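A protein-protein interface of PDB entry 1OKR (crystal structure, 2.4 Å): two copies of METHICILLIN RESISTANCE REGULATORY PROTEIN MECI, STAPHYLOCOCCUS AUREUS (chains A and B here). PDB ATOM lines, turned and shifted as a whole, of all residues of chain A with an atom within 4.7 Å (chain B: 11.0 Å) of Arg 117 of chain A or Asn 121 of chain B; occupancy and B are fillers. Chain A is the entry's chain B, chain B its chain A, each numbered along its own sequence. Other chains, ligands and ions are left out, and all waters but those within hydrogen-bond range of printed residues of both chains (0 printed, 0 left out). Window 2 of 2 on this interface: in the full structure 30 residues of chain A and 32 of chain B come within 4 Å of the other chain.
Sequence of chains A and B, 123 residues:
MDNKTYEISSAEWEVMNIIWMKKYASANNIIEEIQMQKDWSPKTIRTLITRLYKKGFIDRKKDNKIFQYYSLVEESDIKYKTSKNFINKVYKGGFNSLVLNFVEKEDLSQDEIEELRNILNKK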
ATOM      1  N   ILE A 113     -10.095 -30.732 -29.848  1.00  0.00           N
ATOM      2  CA  ILE A 113      -9.137 -29.641 -29.752  1.00  0.00           C
ATOM      3  C   ILE A 113      -9.000 -29.061 -28.321  1.00  0.00           C
ATOM      4  O   ILE A 113      -7.893 -28.708 -27.904  1.00  0.00           O
ATOM      5  CB  ILE A 113      -9.485 -28.525 -30.761  1.00  0.00           C
ATOM      6  CG1 ILE A 113      -9.387 -29.041 -32.204  1.00  0.00           C
ATOM      7  CG2 ILE A 113      -8.567 -27.311 -30.573  1.00  0.00           C
ATOM      8  CD1 ILE A 113      -7.966 -29.073 -32.785  1.00  0.00           C
ATOM      9  N   GLU A 114     -10.098 -28.995 -27.568  1.00  0.00           N
ATOM     10  CA  GLU A 114     -10.088 -28.261 -26.305  1.00  0.00           C
ATOM     11  C   GLU A 114      -9.333 -29.031 -25.242  1.00  0.00           C
ATOM     12  O   GLU A 114      -8.483 -28.464 -24.553  1.00  0.00           O
ATOM     13  CB  GLU A 114     -11.515 -27.901 -25.823  1.00  0.00           C
ATOM     14  CG  GLU A 114     -11.615 -26.623 -24.967  1.00  0.00           C
ATOM     15  CD  GLU A 114     -11.260 -25.321 -25.706  1.00  0.00           C
ATOM     16  OE1 GLU A 114     -11.203 -25.333 -26.955  1.00  0.00           O
ATOM     17  OE2 GLU A 114     -11.037 -24.271 -25.042  1.00  0.00           O
ATOM     18  N   GLU A 115      -9.639 -30.320 -25.115  1.00  0.00           N
ATOM     19  CA  GLU A 115      -8.899 -31.190 -24.197  1.00  0.00           C
ATOM     20  C   GLU A 115      -7.384 -31.117 -24.448  1.00  0.00           C
ATOM     21  O   GLU A 115      -6.612 -31.372 -23.523  1.00  0.00           O
ATOM     22  CB  GLU A 115      -9.385 -32.646 -24.271  1.00  0.00           C
ATOM     23  CG  GLU A 115      -9.218 -33.415 -22.957  1.00  0.00           C
ATOM     24  CD  GLU A 115      -9.061 -34.927 -23.134  1.00  0.00           C
ATOM     25  OE1 GLU A 115      -9.743 -35.511 -24.000  1.00  0.00           O
ATOM     26  OE2 GLU A 115      -8.262 -35.546 -22.395  1.00  0.00           O
ATOM     27  N   LEU A 116      -6.970 -30.769 -25.678  1.00  0.00           N
ATOM     28  CA  LEU A 116      -5.555 -30.524 -25.999  1.00  0.00           C
ATOM     29  C   LEU A 116      -5.104 -29.192 -25.477  1.00  0.00           C
ATOM     30  O   LEU A 116      -4.041 -29.106 -24.887  1.00  0.00           O
ATOM     31  CB  LEU A 116      -5.262 -30.585 -27.511  1.00  0.00           C
ATOM     32  CG  LEU A 116      -5.480 -31.932 -28.214  1.00  0.00           C
ATOM     33  CD1 LEU A 116      -5.109 -31.855 -29.675  1.00  0.00           C
ATOM     34  CD2 LEU A 116      -4.760 -33.084 -27.512  1.00  0.00           C
ATOM     35  N   ARG A 117      -5.894 -28.149 -25.718  1.00  0.00           N
ATOM     36  CA  ARG A 117      -5.652 -26.842 -25.099  1.00  0.00           C
ATOM     37  C   ARG A 117      -5.444 -27.007 -23.596  1.00  0.00           C
ATOM     38  O   ARG A 117      -4.531 -26.434 -23.023  1.00  0.00           O
ATOM     39  CB  ARG A 117      -6.827 -25.887 -25.343  1.00  0.00           C
ATOM     40  CG  ARG A 117      -7.041 -25.488 -26.808  1.00  0.00           C
ATOM     41  CD  ARG A 117      -6.984 -23.971 -27.093  1.00  0.00           C
ATOM     42  NE  ARG A 117      -7.063 -23.731 -28.536  1.00  0.00           N
ATOM     43  CZ  ARG A 117      -8.192 -23.770 -29.244  1.00  0.00           C
ATOM     44  NH1 ARG A 117      -8.165 -23.555 -30.553  1.00  0.00           N
ATOM     45  NH2 ARG A 117      -9.361 -24.013 -28.653  1.00  0.00           N
ATOM     46  N   ASN A 118      -6.287 -27.806 -22.962  1.00  0.00           N
ATOM     47  CA  ASN A 118      -6.261 -27.936 -21.509  1.00  0.00           C
ATOM     48  C   ASN A 118      -5.102 -28.833 -21.055  1.00  0.00           C
ATOM     49  O   ASN A 118      -4.670 -28.783 -19.902  1.00  0.00           O
ATOM     50  CB  ASN A 118      -7.607 -28.465 -20.989  1.00  0.00           C
ATOM     51  CG  ASN A 118      -8.750 -27.425 -21.096  1.00  0.00           C
ATOM     52  OD1 ASN A 118      -9.752 -27.534 -20.386  1.00  0.00           O
ATOM     53  ND2 ASN A 118      -8.598 -26.426 -21.977  1.00  0.00           N
ATOM     54  N   ILE A 119      -4.598 -29.663 -21.968  1.00  0.00           N
ATOM     55  CA  ILE A 119      -3.397 -30.450 -21.692  1.00  0.00           C
ATOM     56  C   ILE A 119      -2.197 -29.506 -21.701  1.00  0.00           C
ATOM     57  O   ILE A 119      -1.255 -29.691 -20.945  1.00  0.00           O
ATOM     58  CB  ILE A 119      -3.257 -31.650 -22.695  1.00  0.00           C
ATOM     59  CG1 ILE A 119      -4.117 -32.837 -22.208  1.00  0.00           C
ATOM     60  CG2 ILE A 119      -1.790 -32.118 -22.820  1.00  0.00           C
ATOM     61  CD1 ILE A 119      -4.380 -33.950 -23.234  1.00  0.00           C
ATOM     62  N   LEU A 120      -2.257 -28.466 -22.519  1.00  0.00           N
ATOM     63  CA  LEU A 120      -1.184 -27.482 -22.575  1.00  0.00           C
ATOM     64  C   LEU A 120      -1.167 -26.596 -21.349  1.00  0.00           C
ATOM     65  O   LEU A 120      -0.172 -26.531 -20.631  1.00  0.00           O
ATOM     66  CB  LEU A 120      -1.327 -26.605 -23.826  1.00  0.00           C
ATOM     67  CG  LEU A 120      -0.470 -26.950 -25.053  1.00  0.00           C
ATOM     68  CD1 LEU A 120      -0.262 -25.715 -25.929  1.00  0.00           C
ATOM     69  CD2 LEU A 120       0.913 -27.591 -24.703  1.00  0.00           C
ATOM     70  N   ASN A 121      -2.300 -25.939 -21.114  1.00  0.00           N
ATOM     71  CA  ASN A 121      -2.394 -24.834 -20.171  1.00  0.00           C
ATOM     72  C   ASN A 121      -2.395 -25.339 -18.736  1.00  0.00           C
ATOM     73  O   ASN A 121      -1.738 -24.754 -17.867  1.00  0.00           O
ATOM     74  CB  ASN A 121      -3.652 -23.992 -20.465  1.00  0.00           C
ATOM     75  CG  ASN A 121      -3.792 -23.648 -21.946  1.00  0.00           C
ATOM     76  OD1 ASN A 121      -2.805 -23.553 -22.672  1.00  0.00           O
ATOM     77  ND2 ASN A 121      -5.018 -23.481 -22.400  1.00  0.00           N
ATOM     78  N   PHE B  95      -4.138 -40.081 -29.487  1.00  0.00           N
ATOM     79  CA  PHE B  95      -3.249 -38.925 -29.624  1.00  0.00           C
ATOM     80  C   PHE B  95      -3.159 -38.058 -28.375  1.00  0.00           C
ATOM     81  O   PHE B  95      -2.123 -37.489 -28.077  1.00  0.00           O
ATOM     82  CB  PHE B  95      -3.693 -38.038 -30.793  1.00  0.00           C
ATOM     83  CG  PHE B  95      -2.795 -36.838 -31.029  1.00  0.00           C
ATOM     84  CD1 PHE B  95      -1.451 -37.010 -31.370  1.00  0.00           C
ATOM     85  CD2 PHE B  95      -3.290 -35.540 -30.915  1.00  0.00           C
ATOM     86  CE1 PHE B  95      -0.630 -35.925 -31.581  1.00  0.00           C
ATOM     87  CE2 PHE B  95      -2.463 -34.425 -31.132  1.00  0.00           C
ATOM     88  CZ  PHE B  95      -1.142 -34.613 -31.475  1.00  0.00           C
ATOM     89  N   ASN B  96      -4.256 -37.981 -27.644  1.00  0.00           N
ATOM     90  CA  ASN B  96      -4.354 -37.133 -26.487  1.00  0.00           C
ATOM     91  C   ASN B  96      -3.530 -37.728 -25.368  1.00  0.00           C
ATOM     92  O   ASN B  96      -2.859 -37.008 -24.660  1.00  0.00           O
ATOM     93  CB  ASN B  96      -5.837 -36.937 -26.112  1.00  0.00           C
ATOM     94  CG  ASN B  96      -6.723 -36.572 -27.357  1.00  0.00           C
ATOM     95  OD1 ASN B  96      -6.893 -37.390 -28.306  1.00  0.00           O
ATOM     96  ND2 ASN B  96      -7.275 -35.350 -27.355  1.00  0.00           N
ATOM     97  N   VAL B  99       0.110 -36.799 -26.143  1.00  0.00           N
ATOM     98  CA  VAL B  99       0.472 -35.445 -25.765  1.00  0.00           C
ATOM     99  C   VAL B  99       0.534 -35.237 -24.246  1.00  0.00           C
ATOM    100  O   VAL B  99       1.385 -34.541 -23.759  1.00  0.00           O
ATOM    101  CB  VAL B  99      -0.448 -34.455 -26.383  1.00  0.00           C
ATOM    102  CG1 VAL B  99      -0.040 -33.051 -25.978  1.00  0.00           C
ATOM    103  CG2 VAL B  99      -0.409 -34.600 -27.911  1.00  0.00           C
ATOM    104  N   LEU B 100      -0.356 -35.880 -23.510  1.00  0.00           N
ATOM    105  CA  LEU B 100      -0.387 -35.802 -22.063  1.00  0.00           C
ATOM    106  C   LEU B 100       0.896 -36.387 -21.552  1.00  0.00           C
ATOM    107  O   LEU B 100       1.517 -35.835 -20.634  1.00  0.00           O
ATOM    108  CB  LEU B 100      -1.580 -36.614 -21.530  1.00  0.00           C
ATOM    109  CG  LEU B 100      -1.828 -36.672 -20.026  1.00  0.00           C
ATOM    110  CD1 LEU B 100      -2.311 -35.312 -19.514  1.00  0.00           C
ATOM    111  CD2 LEU B 100      -2.849 -37.781 -19.722  1.00  0.00           C
ATOM    112  N   VAL B 103       4.060 -33.780 -22.664  1.00  0.00           N
ATOM    113  CA  VAL B 103       3.921 -32.664 -21.748  1.00  0.00           C
ATOM    114  C   VAL B 103       4.152 -33.007 -20.267  1.00  0.00           C
ATOM    115  O   VAL B 103       4.844 -32.279 -19.600  1.00  0.00           O
ATOM    116  CB  VAL B 103       2.525 -32.023 -21.911  1.00  0.00           C
ATOM    117  CG1 VAL B 103       2.256 -31.006 -20.809  1.00  0.00           C
ATOM    118  CG2 VAL B 103       2.403 -31.383 -23.310  1.00  0.00           C
ATOM    119  N   LEU B 108       8.933 -28.205 -21.395  1.00  0.00           N
ATOM    120  CA  LEU B 108       8.772 -27.398 -22.608  1.00  0.00           C
ATOM    121  C   LEU B 108       8.970 -25.927 -22.322  1.00  0.00           C
ATOM    122  O   LEU B 108       8.441 -25.405 -21.346  1.00  0.00           O
ATOM    123  CB  LEU B 108       7.392 -27.601 -23.195  1.00  0.00           C
ATOM    124  CG  LEU B 108       7.137 -28.966 -23.818  1.00  0.00           C
ATOM    125  CD1 LEU B 108       5.658 -29.083 -24.204  1.00  0.00           C
ATOM    126  CD2 LEU B 108       7.998 -29.151 -25.022  1.00  0.00           C
ATOM    127  N   ILE B 113       5.769 -24.017 -25.946  1.00  0.00           N
ATOM    128  CA  ILE B 113       4.375 -23.935 -25.527  1.00  0.00           C
ATOM    129  C   ILE B 113       3.552 -23.039 -26.458  1.00  0.00           C
ATOM    130  O   ILE B 113       2.474 -23.443 -26.827  1.00  0.00           O
ATOM    131  CB  ILE B 113       4.220 -23.491 -24.054  1.00  0.00           C
ATOM    132  CG1 ILE B 113       4.760 -24.540 -23.073  1.00  0.00           C
ATOM    133  CG2 ILE B 113       2.753 -23.330 -23.693  1.00  0.00           C
ATOM    134  CD1 ILE B 113       4.820 -23.987 -21.604  1.00  0.00           C
ATOM    135  N   GLU B 114       4.066 -21.866 -26.853  1.00  0.00           N
ATOM    136  CA  GLU B 114       3.291 -20.885 -27.618  1.00  0.00           C
ATOM    137  C   GLU B 114       3.063 -21.319 -29.048  1.00  0.00           C
ATOM    138  O   GLU B 114       1.978 -21.128 -29.602  1.00  0.00           O
ATOM    139  CB  GLU B 114       3.977 -19.500 -27.680  1.00  0.00           C
ATOM    140  CG  GLU B 114       3.766 -18.498 -26.504  1.00  0.00           C
ATOM    141  CD  GLU B 114       2.431 -18.569 -25.788  1.00  0.00           C
ATOM    142  OE1 GLU B 114       2.391 -18.362 -24.565  1.00  0.00           O
ATOM    143  OE2 GLU B 114       1.414 -18.815 -26.434  1.00  0.00           O
ATOM    144  N   GLU B 115       4.124 -21.830 -29.658  1.00  0.00           N
ATOM    145  CA  GLU B 115       4.086 -22.459 -30.983  1.00  0.00           C
ATOM    146  C   GLU B 115       2.995 -23.508 -31.071  1.00  0.00           C
ATOM    147  O   GLU B 115       2.233 -23.545 -32.057  1.00  0.00           O
ATOM    148  CB  GLU B 115       5.416 -23.146 -31.275  1.00  0.00           C
ATOM    149  CG  GLU B 115       6.152 -22.635 -32.519  1.00  0.00           C
ATOM    150  CD  GLU B 115       6.461 -23.734 -33.525  1.00  0.00           C
ATOM    151  OE1 GLU B 115       7.120 -24.726 -33.145  1.00  0.00           O
ATOM    152  OE2 GLU B 115       6.054 -23.600 -34.702  1.00  0.00           O
ATOM    153  N   LEU B 116       2.916 -24.371 -30.054  1.00  0.00           N
ATOM    154  CA  LEU B 116       1.924 -25.427 -30.077  1.00  0.00           C
ATOM    155  C   LEU B 116       0.543 -24.830 -29.920  1.00  0.00           C
ATOM    156  O   LEU B 116      -0.428 -25.326 -30.469  1.00  0.00           O
ATOM    157  CB  LEU B 116       2.199 -26.464 -28.993  1.00  0.00           C
ATOM    158  CG  LEU B 116       3.475 -27.311 -29.206  1.00  0.00           C
ATOM    159  CD1 LEU B 116       3.999 -27.908 -27.902  1.00  0.00           C
ATOM    160  CD2 LEU B 116       3.251 -28.426 -30.214  1.00  0.00           C
ATOM    161  N   ARG B 117       0.437 -23.755 -29.161  1.00  0.00           N
ATOM    162  CA  ARG B 117      -0.839 -23.064 -29.078  1.00  0.00           C
ATOM    163  C   ARG B 117      -1.199 -22.534 -30.465  1.00  0.00           C
ATOM    164  O   ARG B 117      -2.288 -22.789 -30.958  1.00  0.00           O
ATOM    165  CB  ARG B 117      -0.799 -21.931 -28.050  1.00  0.00           C
ATOM    166  CG  ARG B 117      -1.398 -22.272 -26.716  1.00  0.00           C
ATOM    167  CD  ARG B 117      -1.052 -21.267 -25.627  1.00  0.00           C
ATOM    168  NE  ARG B 117      -1.023 -21.873 -24.293  1.00  0.00           N
ATOM    169  CZ  ARG B 117      -0.314 -21.387 -23.289  1.00  0.00           C
ATOM    170  NH1 ARG B 117      -0.339 -21.977 -22.103  1.00  0.00           N
ATOM    171  NH2 ARG B 117       0.426 -20.305 -23.459  1.00  0.00           N
ATOM    172  N   ASN B 118      -0.266 -21.827 -31.096  1.00  0.00           N
ATOM    173  CA  ASN B 118      -0.441 -21.334 -32.468  1.00  0.00           C
ATOM    174  C   ASN B 118      -0.845 -22.390 -33.500  1.00  0.00           C
ATOM    175  O   ASN B 118      -1.485 -22.062 -34.484  1.00  0.00           O
ATOM    176  CB  ASN B 118       0.828 -20.621 -32.933  1.00  0.00           C
ATOM    177  CG  ASN B 118       1.072 -19.318 -32.180  1.00  0.00           C
ATOM    178  OD1 ASN B 118       0.131 -18.666 -31.707  1.00  0.00           O
ATOM    179  ND2 ASN B 118       2.334 -18.929 -32.071  1.00  0.00           N
ATOM    180  N   ILE B 119      -0.479 -23.644 -33.255  1.00  0.00           N
ATOM    181  CA  ILE B 119      -0.732 -24.753 -34.156  1.00  0.00           C
ATOM    182  C   ILE B 119      -2.167 -25.224 -34.080  1.00  0.00           C
ATOM    183  O   ILE B 119      -2.785 -25.522 -35.122  1.00  0.00           O
ATOM    184  CB  ILE B 119       0.232 -25.895 -33.834  1.00  0.00           C
ATOM    185  CG1 ILE B 119       1.593 -25.619 -34.504  1.00  0.00           C
ATOM    186  CG2 ILE B 119      -0.304 -27.264 -34.309  1.00  0.00           C
ATOM    187  CD1 ILE B 119       2.761 -26.560 -34.048  1.00  0.00           C
ATOM    188  N   LEU B 120      -2.683 -25.312 -32.855  1.00  0.00           N
ATOM    189  CA  LEU B 120      -4.088 -25.665 -32.609  1.00  0.00           C
ATOM    190  C   LEU B 120      -5.017 -24.560 -33.114  1.00  0.00           C
ATOM    191  O   LEU B 120      -5.918 -24.810 -33.930  1.00  0.00           O
ATOM    192  CB  LEU B 120      -4.334 -25.891 -31.114  1.00  0.00           C
ATOM    193  CG  LEU B 120      -3.532 -27.024 -30.457  1.00  0.00           C
ATOM    194  CD1 LEU B 120      -3.632 -27.027 -28.946  1.00  0.00           C
ATOM    195  CD2 LEU B 120      -3.981 -28.350 -30.987  1.00  0.00           C
ATOM    196  N   ASN B 121      -4.757 -23.336 -32.649  1.00  0.00           N
ATOM    197  CA  ASN B 121      -5.487 -22.127 -33.070  1.00  0.00           C
ATOM    198  C   ASN B 121      -5.523 -21.842 -34.592  1.00  0.00           C
ATOM    199  O   ASN B 121      -6.106 -20.841 -34.998  1.00  0.00           O
ATOM    200  CB  ASN B 121      -4.917 -20.887 -32.347  1.00  0.00           C
ATOM    201  CG  ASN B 121      -5.328 -20.800 -30.873  1.00  0.00           C
ATOM    202  OD1 ASN B 121      -6.147 -21.581 -30.381  1.00  0.00           O
ATOM    203  ND2 ASN B 121      -4.740 -19.843 -30.162  1.00  0.00           N
ATOM    204  N   LYS B 122      -4.904 -22.691 -35.421  1.00  0.00           N
ATOM    205  CA  LYS B 122      -4.990 -22.568 -36.885  1.00  0.00           C
ATOM    206  C   LYS B 122      -6.082 -23.508 -37.477  1.00  0.00           C
ATOM    207  O   LYS B 122      -5.904 -24.095 -38.551  1.00  0.00           O
ATOM    208  CB  LYS B 122      -3.599 -22.808 -37.527  1.00  0.00           C
ATOM    209  CG  LYS B 122      -2.997 -21.578 -38.258  1.00  0.00           C
ATOM    210  CD  LYS B 122      -2.474 -20.508 -37.291  1.00  0.00           C
ATOM    211  CE  LYS B 122      -0.959 -20.434 -37.289  1.00  0.00           C
ATOM    212  NZ  LYS B 122      -0.442 -19.760 -36.069  1.00  0.00           N
ATOM    213  N   LYS B 123      -7.223 -23.607 -36.779  1.00  0.00           N
ATOM    214  CA  LYS B 123      -8.350 -24.488 -37.148  1.00  0.00           C
ATOM    215  C   LYS B 123      -7.920 -25.964 -37.330  1.00  0.00           C
ATOM    216  O   LYS B 123      -7.118 -26.508 -36.559  1.00  0.00           O
ATOM    217  CB  LYS B 123      -9.116 -23.939 -38.378  1.00  0.00           C
ATOM    218  CG  LYS B 123     -10.405 -23.152 -38.041  1.00  0.00           C
ATOM    219  CD  LYS B 123     -11.309 -22.972 -39.269  1.00  0.00           C
ATOM    220  CE  LYS B 123     -12.796 -23.117 -38.948  1.00  0.00           C
ATOM    221  NZ  LYS B 123     -13.393 -24.300 -39.625  1.00  0.00           N
ATOM    222  OXT LYS B 123      -8.353 -26.696 -38.225  1.00  0.00           O
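The side-chain amide nitrogen (ND2) of Asn 121 of chain A lies within hydrogen-bond range of the backbone carbonyl oxygen (O) of Arg 117 of chain A (3.1 Å). NH2 of Arg 117 of chain B lies within salt-bridge range of OE1 of Glu 114 of chain B. The side-chain carboxylate (OE1) of Glu 114 of chain A is in salt-bridge range of the guanidinium group (NH2) of Arg 117 of chain A, at 2.8 Å.
The guanidinium group of Arg 117 of chain B sits at hydrogen-bond distance from the side-chain amide oxygen of Asn 121 of chain A (2.9 Å). NH1 of Arg 117 of chain A lies within hydrogen-bond range of OD1 of Asn 121 of chain B (2.8 Å).
No residue of chain B comes within 4 Å of Glu 114 of chain A. Arg 117 of chain A touches one residue of chain B. Of the printed residues of chain B, Leu 120 of chain A touches Ile 113 and Arg 117. Printed residues of chain A within 4 Å of Phe 95 of chain B: Leu 116. Of the printed residues of chain A, Asn 96 of chain B touches Leu 116 and Ile 119. Leu 108 of chain B touches none of the printed residues of chain A. Printed residues of chain A within 4 Å of Ile 113 of chain B: Leu 120 (3.7 Å). Of the printed residues of chain A, Leu 120 of chain B touches Leu 116. Printed residues of chain A within 4 Å of Asn 121 of chain B: Arg 117. Lys 123 of chain B touches none of the printed residues of chain A. The nearest residue of chain B that does not touch Arg 117 of chain A is Leu 120 of chain B (4.1 Å).
Among the printed residues, pairs that only touch across the chains: Leu 116 of chain A with Phe 95 of chain B, Leu 116 of chain A with Asn 96 of chain B, Leu 116 of chain A with Leu 120 of chain B, Ile 119 of chain A with Asn 96 of chain B, Ile 119 of chain A with Val 99 of chain B, Ile 119 of chain A with Val 103 of chain B, Leu 120 of chain A with Ile 113 of chain B and Leu 120 of chain A with Arg 117 of chain B.
Leu 116 of chain A touches Leu 120 of chain B, but with the chains exchanged Leu 120 of chain A does not touch Leu 116 of chain B (4.001 Å). Arg 117 of chain A touches Asn 121 of chain B, and with the chains exchanged Asn 121 of chain A touches Arg 117 of chain B. Leu 120 of chain A touches Ile 113 of chain B, but with the chains exchanged Ile 113 of chain A does not touch Leu 120 of chain B (4.4 Å). Leu 120 of chain A touches Arg 117 of chain B, but with the chains exchanged Arg 117 of chain A does not touch Leu 120 of chain B (4.1 Å). Positions printed for both chains: 113, 114, 115, 116, 117, 118, 119, 120 and 121.
Of the 9 printed residues of chain A, 5 touch a printed residue of chain B. Printed residues of chain A that touch a printed residue of chain B: Leu 116, Arg 117, Ile 119, Leu 120 and Asn 121. Among the printed residues, 10 pairs touch across the chains.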
